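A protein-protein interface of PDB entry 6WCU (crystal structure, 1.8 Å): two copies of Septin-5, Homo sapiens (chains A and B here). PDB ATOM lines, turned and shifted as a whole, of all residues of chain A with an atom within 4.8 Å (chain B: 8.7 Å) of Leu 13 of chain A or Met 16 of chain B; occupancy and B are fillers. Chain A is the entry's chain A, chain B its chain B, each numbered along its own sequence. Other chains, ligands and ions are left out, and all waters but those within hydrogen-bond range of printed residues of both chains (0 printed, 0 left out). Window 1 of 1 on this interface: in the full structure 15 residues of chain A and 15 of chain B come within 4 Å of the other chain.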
ATOM      1  N   LYS A   9     -13.449 -26.649   2.348  1.00  0.00           N
ATOM      2  CA  LYS A   9     -13.575 -25.343   2.977  1.00  0.00           C
ATOM      3  C   LYS A   9     -12.263 -24.578   2.931  1.00  0.00           C
ATOM      4  O   LYS A   9     -12.275 -23.348   2.875  1.00  0.00           O
ATOM      5  CB  LYS A   9     -14.069 -25.490   4.416  1.00  0.00           C
ATOM      6  CG  LYS A   9     -15.484 -26.000   4.509  1.00  0.00           C
ATOM      7  CD  LYS A   9     -15.891 -26.263   5.932  1.00  0.00           C
ATOM      8  CE  LYS A   9     -17.168 -27.083   5.976  1.00  0.00           C
ATOM      9  NZ  LYS A   9     -18.319 -26.346   5.385  1.00  0.00           N
ATOM     10  N   ASP A  10     -11.129 -25.278   2.935  1.00  0.00           N
ATOM     11  CA  ASP A  10      -9.855 -24.589   2.765  1.00  0.00           C
ATOM     12  C   ASP A  10      -9.711 -24.015   1.358  1.00  0.00           C
ATOM     13  O   ASP A  10      -9.135 -22.935   1.186  1.00  0.00           O
ATOM     14  CB  ASP A  10      -8.697 -25.532   3.092  1.00  0.00           C
ATOM     15  CG  ASP A  10      -8.503 -25.702   4.579  1.00  0.00           C
ATOM     16  OD1 ASP A  10      -8.960 -24.815   5.324  1.00  0.00           O
ATOM     17  OD2 ASP A  10      -7.881 -26.696   5.002  1.00  0.00           O
ATOM     18  N   GLU A  11     -10.222 -24.711   0.339  1.00  0.00           N
ATOM     19  CA  GLU A  11     -10.195 -24.130  -1.000  1.00  0.00           C
ATOM     20  C   GLU A  11     -11.108 -22.913  -1.095  1.00  0.00           C
ATOM     21  O   GLU A  11     -10.733 -21.894  -1.685  1.00  0.00           O
ATOM     22  CB  GLU A  11     -10.588 -25.164  -2.052  1.00  0.00           C
ATOM     23  CG  GLU A  11     -10.713 -24.566  -3.455  1.00  0.00           C
ATOM     24  CD  GLU A  11     -11.250 -25.543  -4.481  1.00  0.00           C
ATOM     25  OE1 GLU A  11     -11.326 -26.752  -4.178  1.00  0.00           O
ATOM     26  OE2 GLU A  11     -11.615 -25.099  -5.591  1.00  0.00           O
ATOM     27  N   GLU A  12     -12.302 -22.993  -0.502  1.00  0.00           N
ATOM     28  CA  GLU A  12     -13.222 -21.864  -0.557  1.00  0.00           C
ATOM     29  C   GLU A  12     -12.643 -20.656   0.157  1.00  0.00           C
ATOM     30  O   GLU A  12     -12.750 -19.530  -0.333  1.00  0.00           O
ATOM     31  CB  GLU A  12     -14.570 -22.229   0.050  1.00  0.00           C
ATOM     32  CG  GLU A  12     -15.651 -21.257  -0.353  1.00  0.00           C
ATOM     33  CD  GLU A  12     -17.020 -21.666   0.121  1.00  0.00           C
ATOM     34  OE1 GLU A  12     -17.128 -22.204   1.241  1.00  0.00           O
ATOM     35  OE2 GLU A  12     -17.988 -21.494  -0.653  1.00  0.00           O
ATOM     36  N   LEU A  13     -12.039 -20.864   1.324  1.00  0.00           N
ATOM     37  CA  LEU A  13     -11.395 -19.756   2.018  1.00  0.00           C
ATOM     38  C   LEU A  13     -10.331 -19.119   1.142  1.00  0.00           C
ATOM     39  O   LEU A  13     -10.207 -17.892   1.102  1.00  0.00           O
ATOM     40  CB  LEU A  13     -10.786 -20.233   3.338  1.00  0.00           C
ATOM     41  CG  LEU A  13     -11.787 -20.418   4.474  1.00  0.00           C
ATOM     42  CD1 LEU A  13     -11.162 -21.149   5.652  1.00  0.00           C
ATOM     43  CD2 LEU A  13     -12.334 -19.072   4.889  1.00  0.00           C
ATOM     44  N   ARG A  14      -9.585 -19.919   0.398  1.00  0.00           N
ATOM     45  CA  ARG A  14      -8.571 -19.347  -0.464  1.00  0.00           C
ATOM     46  C   ARG A  14      -9.228 -18.515  -1.574  1.00  0.00           C
ATOM     47  O   ARG A  14      -8.795 -17.413  -1.837  1.00  0.00           O
ATOM     48  CB  ARG A  14      -7.668 -20.421  -1.039  1.00  0.00           C
ATOM     49  CG  ARG A  14      -6.764 -19.958  -2.150  1.00  0.00           C
ATOM     50  CD  ARG A  14      -6.111 -21.146  -2.833  1.00  0.00           C
ATOM     51  NE  ARG A  14      -7.022 -21.886  -3.707  1.00  0.00           N
ATOM     52  CZ  ARG A  14      -7.414 -21.473  -4.911  1.00  0.00           C
ATOM     53  NH1 ARG A  14      -8.238 -22.215  -5.618  1.00  0.00           N
ATOM     54  NH2 ARG A  14      -6.999 -20.326  -5.399  1.00  0.00           N
ATOM     55  N   ARG A  15     -10.331 -18.998  -2.131  1.00  0.00           N
ATOM     56  CA  ARG A  15     -11.018 -18.256  -3.181  1.00  0.00           C
ATOM     57  C   ARG A  15     -11.548 -16.937  -2.648  1.00  0.00           C
ATOM     58  O   ARG A  15     -11.409 -15.895  -3.296  1.00  0.00           O
ATOM     59  CB  ARG A  15     -12.170 -19.097  -3.731  1.00  0.00           C
ATOM     60  CG  ARG A  15     -11.745 -20.425  -4.307  1.00  0.00           C
ATOM     61  CD  ARG A  15     -11.295 -20.282  -5.727  1.00  0.00           C
ATOM     62  NE  ARG A  15     -12.402 -19.902  -6.589  1.00  0.00           N
ATOM     63  CZ  ARG A  15     -13.095 -20.762  -7.322  1.00  0.00           C
ATOM     64  NH1 ARG A  15     -14.095 -20.337  -8.081  1.00  0.00           N
ATOM     65  NH2 ARG A  15     -12.778 -22.049  -7.299  1.00  0.00           N
ATOM     66  N   MET A  16     -12.147 -16.961  -1.457  1.00  0.00           N
ATOM     67  CA  MET A  16     -12.715 -15.739  -0.901  1.00  0.00           C
ATOM     68  C   MET A  16     -11.637 -14.740  -0.508  1.00  0.00           C
ATOM     69  O   MET A  16     -11.854 -13.531  -0.603  1.00  0.00           O
ATOM     70  CB  MET A  16     -13.599 -16.061   0.300  1.00  0.00           C
ATOM     71  CG  MET A  16     -14.765 -16.957  -0.030  1.00  0.00           C
ATOM     72  SD  MET A  16     -15.840 -17.133   1.394  1.00  0.00           S
ATOM     73  CE  MET A  16     -16.312 -15.438   1.637  1.00  0.00           C
ATOM     74  N   GLN A  17     -10.477 -15.214  -0.061  1.00  0.00           N
ATOM     75  CA  GLN A  17      -9.403 -14.274   0.231  1.00  0.00           C
ATOM     76  C   GLN A  17      -8.832 -13.693  -1.056  1.00  0.00           C
ATOM     77  O   GLN A  17      -8.524 -12.500  -1.119  1.00  0.00           O
ATOM     78  CB  GLN A  17      -8.317 -14.947   1.070  1.00  0.00           C
ATOM     79  CG  GLN A  17      -7.276 -13.978   1.557  1.00  0.00           C
ATOM     80  CD  GLN A  17      -6.528 -14.486   2.762  1.00  0.00           C
ATOM     81  OE1 GLN A  17      -7.127 -14.935   3.733  1.00  0.00           O
ATOM     82  NE2 GLN A  17      -5.208 -14.417   2.706  1.00  0.00           N
ATOM     83  N   LEU A  20     -11.223 -11.080  -1.993  1.00  0.00           N
ATOM     84  CA  LEU A  20     -10.988  -9.903  -1.162  1.00  0.00           C
ATOM     85  C   LEU A  20      -9.799  -9.101  -1.666  1.00  0.00           C
ATOM     86  O   LEU A  20      -9.821  -7.867  -1.641  1.00  0.00           O
ATOM     87  CB  LEU A  20     -10.751 -10.317   0.286  1.00  0.00           C
ATOM     88  CG  LEU A  20     -11.946 -10.622   1.179  1.00  0.00           C
ATOM     89  CD1 LEU A  20     -11.454 -11.233   2.475  1.00  0.00           C
ATOM     90  CD2 LEU A  20     -12.715  -9.358   1.457  1.00  0.00           C
ATOM     91  N   LEU B   5     -12.362 -28.154  13.820  1.00  0.00           N
ATOM     92  CA  LEU B   5     -11.818 -27.429  12.673  1.00  0.00           C
ATOM     93  C   LEU B   5     -12.910 -27.016  11.698  1.00  0.00           C
ATOM     94  O   LEU B   5     -12.898 -25.896  11.181  1.00  0.00           O
ATOM     95  CB  LEU B   5     -10.788 -28.288  11.949  1.00  0.00           C
ATOM     96  CG  LEU B   5      -9.350 -28.191  12.426  1.00  0.00           C
ATOM     97  CD1 LEU B   5      -8.491 -29.174  11.657  1.00  0.00           C
ATOM     98  CD2 LEU B   5      -8.877 -26.769  12.212  1.00  0.00           C
ATOM     99  N   ILE B   6     -13.847 -27.916  11.418  1.00  0.00           N
ATOM    100  CA  ILE B   6     -14.914 -27.601  10.475  1.00  0.00           C
ATOM    101  C   ILE B   6     -15.702 -26.400  10.963  1.00  0.00           C
ATOM    102  O   ILE B   6     -16.078 -25.525  10.177  1.00  0.00           O
ATOM    103  CB  ILE B   6     -15.812 -28.830  10.260  1.00  0.00           C
ATOM    104  CG1 ILE B   6     -15.066 -29.884   9.444  1.00  0.00           C
ATOM    105  CG2 ILE B   6     -17.079 -28.451   9.547  1.00  0.00           C
ATOM    106  CD1 ILE B   6     -15.850 -31.161   9.225  1.00  0.00           C
ATOM    107  N   MET B   8     -14.540 -24.027  12.963  1.00  0.00           N
ATOM    108  CA  MET B   8     -13.665 -22.865  12.838  1.00  0.00           C
ATOM    109  C   MET B   8     -13.641 -22.343  11.408  1.00  0.00           C
ATOM    110  O   MET B   8     -13.721 -21.135  11.175  1.00  0.00           O
ATOM    111  CB  MET B   8     -12.251 -23.222  13.283  1.00  0.00           C
ATOM    112  CG  MET B   8     -12.069 -23.439  14.765  1.00  0.00           C
ATOM    113  SD  MET B   8     -10.414 -24.087  15.060  1.00  0.00           S
ATOM    114  CE  MET B   8      -9.458 -23.005  14.007  1.00  0.00           C
ATOM    115  N   LYS B   9     -13.500 -23.241  10.435  1.00  0.00           N
ATOM    116  CA  LYS B   9     -13.457 -22.804   9.047  1.00  0.00           C
ATOM    117  C   LYS B   9     -14.825 -22.336   8.573  1.00  0.00           C
ATOM    118  O   LYS B   9     -14.911 -21.501   7.673  1.00  0.00           O
ATOM    119  CB  LYS B   9     -12.922 -23.925   8.163  1.00  0.00           C
ATOM    120  CG  LYS B   9     -11.483 -24.257   8.457  1.00  0.00           C
ATOM    121  CD  LYS B   9     -11.030 -25.457   7.667  1.00  0.00           C
ATOM    122  CE  LYS B   9      -9.720 -26.013   8.204  1.00  0.00           C
ATOM    123  NZ  LYS B   9      -8.585 -25.059   8.071  1.00  0.00           N
ATOM    124  N   ASP B  10     -15.903 -22.871   9.140  1.00  0.00           N
ATOM    125  CA  ASP B  10     -17.212 -22.320   8.825  1.00  0.00           C
ATOM    126  C   ASP B  10     -17.373 -20.915   9.394  1.00  0.00           C
ATOM    127  O   ASP B  10     -18.025 -20.076   8.769  1.00  0.00           O
ATOM    128  CB  ASP B  10     -18.318 -23.249   9.323  1.00  0.00           C
ATOM    129  CG  ASP B  10     -18.508 -24.450   8.416  1.00  0.00           C
ATOM    130  OD1 ASP B  10     -18.099 -24.353   7.242  1.00  0.00           O
ATOM    131  OD2 ASP B  10     -19.082 -25.472   8.852  1.00  0.00           O
ATOM    132  N   GLU B  11     -16.787 -20.636  10.566  1.00  0.00           N
ATOM    133  CA  GLU B  11     -16.821 -19.278  11.110  1.00  0.00           C
ATOM    134  C   GLU B  11     -16.013 -18.310  10.249  1.00  0.00           C
ATOM    135  O   GLU B  11     -16.439 -17.174  10.016  1.00  0.00           O
ATOM    136  CB  GLU B  11     -16.314 -19.268  12.554  1.00  0.00           C
ATOM    137  CG  GLU B  11     -16.187 -17.874  13.162  1.00  0.00           C
ATOM    138  CD  GLU B  11     -15.539 -17.870  14.540  1.00  0.00           C
ATOM    139  OE1 GLU B  11     -15.367 -18.955  15.130  1.00  0.00           O
ATOM    140  OE2 GLU B  11     -15.189 -16.777  15.035  1.00  0.00           O
ATOM    141  N   GLU B  12     -14.843 -18.745   9.771  1.00  0.00           N
ATOM    142  CA  GLU B  12     -14.023 -17.901   8.908  1.00  0.00           C
ATOM    143  C   GLU B  12     -14.739 -17.584   7.603  1.00  0.00           C
ATOM    144  O   GLU B  12     -14.736 -16.437   7.152  1.00  0.00           O
ATOM    145  CB  GLU B  12     -12.694 -18.589   8.609  1.00  0.00           C
ATOM    146  CG  GLU B  12     -11.630 -17.694   8.012  1.00  0.00           C
ATOM    147  CD  GLU B  12     -10.302 -18.411   7.837  1.00  0.00           C
ATOM    148  OE1 GLU B  12     -10.142 -19.509   8.407  1.00  0.00           O
ATOM    149  OE2 GLU B  12      -9.430 -17.895   7.105  1.00  0.00           O
ATOM    150  N   LEU B  13     -15.360 -18.588   6.986  1.00  0.00           N
ATOM    151  CA  LEU B  13     -16.110 -18.361   5.754  1.00  0.00           C
ATOM    152  C   LEU B  13     -17.210 -17.328   5.953  1.00  0.00           C
ATOM    153  O   LEU B  13     -17.464 -16.506   5.067  1.00  0.00           O
ATOM    154  CB  LEU B  13     -16.703 -19.678   5.249  1.00  0.00           C
ATOM    155  CG  LEU B  13     -15.760 -20.631   4.516  1.00  0.00           C
ATOM    156  CD1 LEU B  13     -16.383 -22.001   4.348  1.00  0.00           C
ATOM    157  CD2 LEU B  13     -15.405 -20.055   3.172  1.00  0.00           C
ATOM    158  N   ARG B  14     -17.881 -17.362   7.104  1.00  0.00           N
ATOM    159  CA  ARG B  14     -18.927 -16.381   7.372  1.00  0.00           C
ATOM    160  C   ARG B  14     -18.358 -14.971   7.491  1.00  0.00           C
ATOM    161  O   ARG B  14     -18.916 -14.024   6.927  1.00  0.00           O
ATOM    162  CB  ARG B  14     -19.698 -16.773   8.633  1.00  0.00           C
ATOM    163  CG  ARG B  14     -20.515 -18.051   8.461  1.00  0.00           C
ATOM    164  CD  ARG B  14     -21.485 -18.283   9.611  1.00  0.00           C
ATOM    165  NE  ARG B  14     -20.825 -18.837  10.788  1.00  0.00           N
ATOM    166  CZ  ARG B  14     -20.832 -20.124  11.106  1.00  0.00           C
ATOM    167  NH1 ARG B  14     -21.467 -20.986  10.331  1.00  0.00           N
ATOM    168  NH2 ARG B  14     -20.208 -20.548  12.197  1.00  0.00           N
ATOM    169  N   ARG B  15     -17.241 -14.810   8.206  1.00  0.00           N
ATOM    170  CA  ARG B  15     -16.663 -13.481   8.384  1.00  0.00           C
ATOM    171  C   ARG B  15     -16.140 -12.916   7.070  1.00  0.00           C
ATOM    172  O   ARG B  15     -16.327 -11.730   6.785  1.00  0.00           O
ATOM    173  CB  ARG B  15     -15.566 -13.521   9.451  1.00  0.00           C
ATOM    174  CG  ARG B  15     -16.092 -13.931  10.827  1.00  0.00           C
ATOM    175  CD  ARG B  15     -15.104 -13.658  11.947  1.00  0.00           C
ATOM    176  NE  ARG B  15     -14.331 -14.848  12.286  1.00  0.00           N
ATOM    177  CZ  ARG B  15     -13.509 -14.944  13.329  1.00  0.00           C
ATOM    178  NH1 ARG B  15     -13.347 -13.915  14.152  1.00  0.00           N
ATOM    179  NH2 ARG B  15     -12.853 -16.074  13.551  1.00  0.00           N
ATOM    180  N   MET B  16     -15.492 -13.745   6.252  1.00  0.00           N
ATOM    181  CA  MET B  16     -15.003 -13.253   4.968  1.00  0.00           C
ATOM    182  C   MET B  16     -16.141 -12.880   4.030  1.00  0.00           C
ATOM    183  O   MET B  16     -15.961 -12.008   3.172  1.00  0.00           O
ATOM    184  CB  MET B  16     -14.101 -14.287   4.301  1.00  0.00           C
ATOM    185  CG  MET B  16     -12.674 -14.279   4.793  1.00  0.00           C
ATOM    186  SD  MET B  16     -11.692 -15.453   3.861  1.00  0.00           S
ATOM    187  CE  MET B  16     -10.131 -15.341   4.720  1.00  0.00           C
ATOM    188  N   GLN B  17     -17.305 -13.515   4.162  1.00  0.00           N
ATOM    189  CA  GLN B  17     -18.425 -13.141   3.307  1.00  0.00           C
ATOM    190  C   GLN B  17     -19.063 -11.842   3.774  1.00  0.00           C
ATOM    191  O   GLN B  17     -19.393 -10.984   2.950  1.00  0.00           O
ATOM    192  CB  GLN B  17     -19.449 -14.274   3.251  1.00  0.00           C
ATOM    193  CG  GLN B  17     -20.551 -14.032   2.248  1.00  0.00           C
ATOM    194  CD  GLN B  17     -21.221 -15.306   1.809  1.00  0.00           C
ATOM    195  OE1 GLN B  17     -20.557 -16.274   1.436  1.00  0.00           O
ATOM    196  NE2 GLN B  17     -22.544 -15.325   1.865  1.00  0.00           N
ATOM    197  N   GLU B  18     -19.216 -11.664   5.085  1.00  0.00           N
ATOM    198  CA  GLU B  18     -19.641 -10.369   5.601  1.00  0.00           C
ATOM    199  C   GLU B  18     -18.694  -9.271   5.141  1.00  0.00           C
ATOM    200  O   GLU B  18     -19.133  -8.176   4.781  1.00  0.00           O
ATOM    201  CB  GLU B  18     -19.709 -10.405   7.130  1.00  0.00           C
ATOM    202  CG  GLU B  18     -20.799 -11.299   7.707  1.00  0.00           C
ATOM    203  CD  GLU B  18     -20.611 -11.550   9.196  1.00  0.00           C
ATOM    204  OE1 GLU B  18     -19.484 -11.357   9.699  1.00  0.00           O
ATOM    205  OE2 GLU B  18     -21.593 -11.926   9.865  1.00  0.00           O
ATOM    206  N   MET B  19     -17.392  -9.555   5.127  1.00  0.00           N
ATOM    207  CA  MET B  19     -16.409  -8.562   4.710  1.00  0.00           C
ATOM    208  C   MET B  19     -16.505  -8.262   3.220  1.00  0.00           C
ATOM    209  O   MET B  19     -16.345  -7.111   2.803  1.00  0.00           O
ATOM    210  CB  MET B  19     -15.010  -9.060   5.048  1.00  0.00           C
ATOM    211  CG  MET B  19     -13.917  -8.046   4.850  1.00  0.00           C
ATOM    212  SD  MET B  19     -12.371  -8.795   5.358  1.00  0.00           S
ATOM    213  CE  MET B  19     -12.874  -9.453   6.943  1.00  0.00           C
ATOM    214  N   LEU B  20     -16.753  -9.287   2.405  1.00  0.00           N
ATOM    215  CA  LEU B  20     -16.928  -9.076   0.972  1.00  0.00           C
ATOM    216  C   LEU B  20     -18.154  -8.224   0.684  1.00  0.00           C
ATOM    217  O   LEU B  20     -18.095  -7.290  -0.121  1.00  0.00           O
ATOM    218  CB  LEU B  20     -17.028 -10.421   0.257  1.00  0.00           C
ATOM    219  CG  LEU B  20     -15.701 -11.118  -0.018  1.00  0.00           C
ATOM    220  CD1 LEU B  20     -15.976 -12.526  -0.486  1.00  0.00           C
ATOM    221  CD2 LEU B  20     -14.911 -10.360  -1.056  1.00  0.00           C
ATOM    222  N   GLN B  21     -19.283  -8.535   1.322  1.00  0.00           N
ATOM    223  CA  GLN B  21     -20.463  -7.705   1.136  1.00  0.00           C
ATOM    224  C   GLN B  21     -20.307  -6.341   1.792  1.00  0.00           C
ATOM    225  O   GLN B  21     -20.987  -5.392   1.391  1.00  0.00           O
ATOM    226  CB  GLN B  21     -21.702  -8.413   1.689  1.00  0.00           C
ATOM    227  CG  GLN B  21     -21.665  -8.646   3.190  1.00  0.00           C
ATOM    228  CD  GLN B  21     -22.906  -9.347   3.702  1.00  0.00           C
ATOM    229  OE1 GLN B  21     -23.627  -9.986   2.934  1.00  0.00           O
ATOM    230  NE2 GLN B  21     -23.158  -9.234   5.002  1.00  0.00           N
ATOM    231  N   ARG B  22     -19.412  -6.222   2.776  1.00  0.00           N
ATOM    232  CA  ARG B  22     -19.090  -4.917   3.343  1.00  0.00           C
ATOM    233  C   ARG B  22     -18.227  -4.104   2.385  1.00  0.00           C
ATOM    234  O   ARG B  22     -18.445  -2.901   2.215  1.00  0.00           O
ATOM    235  CB  ARG B  22     -18.388  -5.105   4.688  1.00  0.00           C
ATOM    236  CG  ARG B  22     -18.229  -3.854   5.515  1.00  0.00           C
ATOM    237  CD  ARG B  22     -18.128  -4.178   7.005  1.00  0.00           C
ATOM    238  NE  ARG B  22     -17.093  -5.161   7.315  1.00  0.00           N
ATOM    239  CZ  ARG B  22     -17.333  -6.400   7.738  1.00  0.00           C
ATOM    240  NH1 ARG B  22     -18.578  -6.824   7.908  1.00  0.00           N
ATOM    241  NH2 ARG B  22     -16.322  -7.216   7.995  1.00  0.00           N
ATOM    242  N   MET B  23     -17.250  -4.749   1.745  1.00  0.00           N
ATOM    243  CA  MET B  23     -16.467  -4.073   0.717  1.00  0.00           C
ATOM    244  C   MET B  23     -17.308  -3.762  -0.509  1.00  0.00           C
ATOM    245  O   MET B  23     -17.042  -2.780  -1.209  1.00  0.00           O
ATOM    246  CB  MET B  23     -15.277  -4.933   0.310  1.00  0.00           C
ATOM    247  CG  MET B  23     -14.264  -5.142   1.408  1.00  0.00           C
ATOM    248  SD  MET B  23     -12.837  -6.032   0.797  1.00  0.00           S
ATOM    249  CE  MET B  23     -12.225  -4.872  -0.417  1.00  0.00           C
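The side-chain amino group (NZ) of Lys 9 of chain A is in salt-bridge range of the side-chain carboxylate (OD1) of Asp 10 of chain B. NZ of Lys 9 of chain B lies within salt-bridge range of OD1 of Asp 10 of chain A, 2.8 Å away.
Of the 10 printed residues of chain A, 7 touch a printed residue of chain B. Printed residues of chain A that touch a printed residue of chain B: Lys 9, Asp 10, Glu 12, Leu 13, Met 16, Gln 17 and Leu 20. Hydrophobic or aromatic side chains of chain A within 4 Å of the printed part of chain B: Leu 13, Met 16 and Leu 20. Of the 18 printed residues of chain B, 10 touch a printed residue of chain A. Hydrophobic or aromatic side chains of chain B that line the printed part of chain A: Ile 6, Leu 13, Met 16, Met 19, Leu 20 and Met 23. Among the printed residues, Asp or Glu carboxylates within 4 Å of a Lys or Arg side-chain nitrogen of the other chain: Lys 9 of chain A with Asp 10 of chain B (2.7 Å) and Asp 10 of chain A with Lys 9 of chain B (2.8 Å).
CE of Lys 9 of chain A touches CG2 of Ile 6 of chain B, 3.8 Å away. Glu 12 of chain A touches Leu 13 of chain B (OE1 to CD1, 3.2 Å). Leu 13 of chain A touches Leu 13 of chain B. Leu 13 of chain A touches Met 16 of chain B (CD2 to SD, 3.8 Å). Met 16 of chain A touches Leu 13 of chain B. CE of Met 16 of chain A touches C of Met 16 of chain B (3.5 Å). Met 16 of chain A touches Leu 20 of chain B (CE to CD1, 3.6 Å). Gln 17 of chain A touches Met 16 of chain B (OE1 to CE, 3.2 Å). Met 19 of chain B touches Leu 20 of chain A. Leu 20 of chain A touches Leu 20 of chain B.
Glu 12 of chain A touches Leu 13 of chain B, and with the chains exchanged Leu 13 of chain A touches Glu 12 of chain B. Leu 13 of chain A touches Met 16 of chain B, and with the chains exchanged Met 16 of chain A touches Leu 13 of chain B. Met 16 of chain B touches its own counterpart, Met 16 of chain A. Met 16 of chain A touches Gln 17 of chain B, and with the chains exchanged Gln 17 of chain A touches Met 16 of chain B. 10 positions are printed for both chains. Of the 15 pairs that touch across the chains among the printed residues, 11 have their exchanged pair printed and touching as well.
Printed residues of chain B within 4 Å of Leu 13 of chain A: Glu 12 (3.4 Å), Leu 13 (3.7 Å) and Met 16 (3.8 Å). Printed residues of chain A within 4 Å of Met 16 of chain B: Leu 13, Met 16 and Gln 17. Of the printed residues of chain A, Met 23 of chain B touches Leu 20. Of the printed residues of chain A, Glu 12 of chain B touches Leu 13 (3.4 Å). Printed residues of chain A within 4 Å of Lys 9 of chain B: Asp 10. Of the printed residues of chain A, Ile 6 of chain B touches Lys 9. Of the printed residues of chain A, Gln 17 of chain B touches Met 16 (3.3 Å). Arg 15 of chain B touches none of the printed residues of chain A. Glu 11 of chain B touches none of the printed residues of chain A. The nearest printed residue of chain B that does not touch Leu 13 of chain A is Lys 9 of chain B (4.1 Å). The nearest printed residue of chain A that does not touch Met 16 of chain B is Leu 20 of chain A (4.02 Å). The nearest printed residue of chain B that does not touch Lys 9 of chain A is Leu 13 of chain B (4.1 Å).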
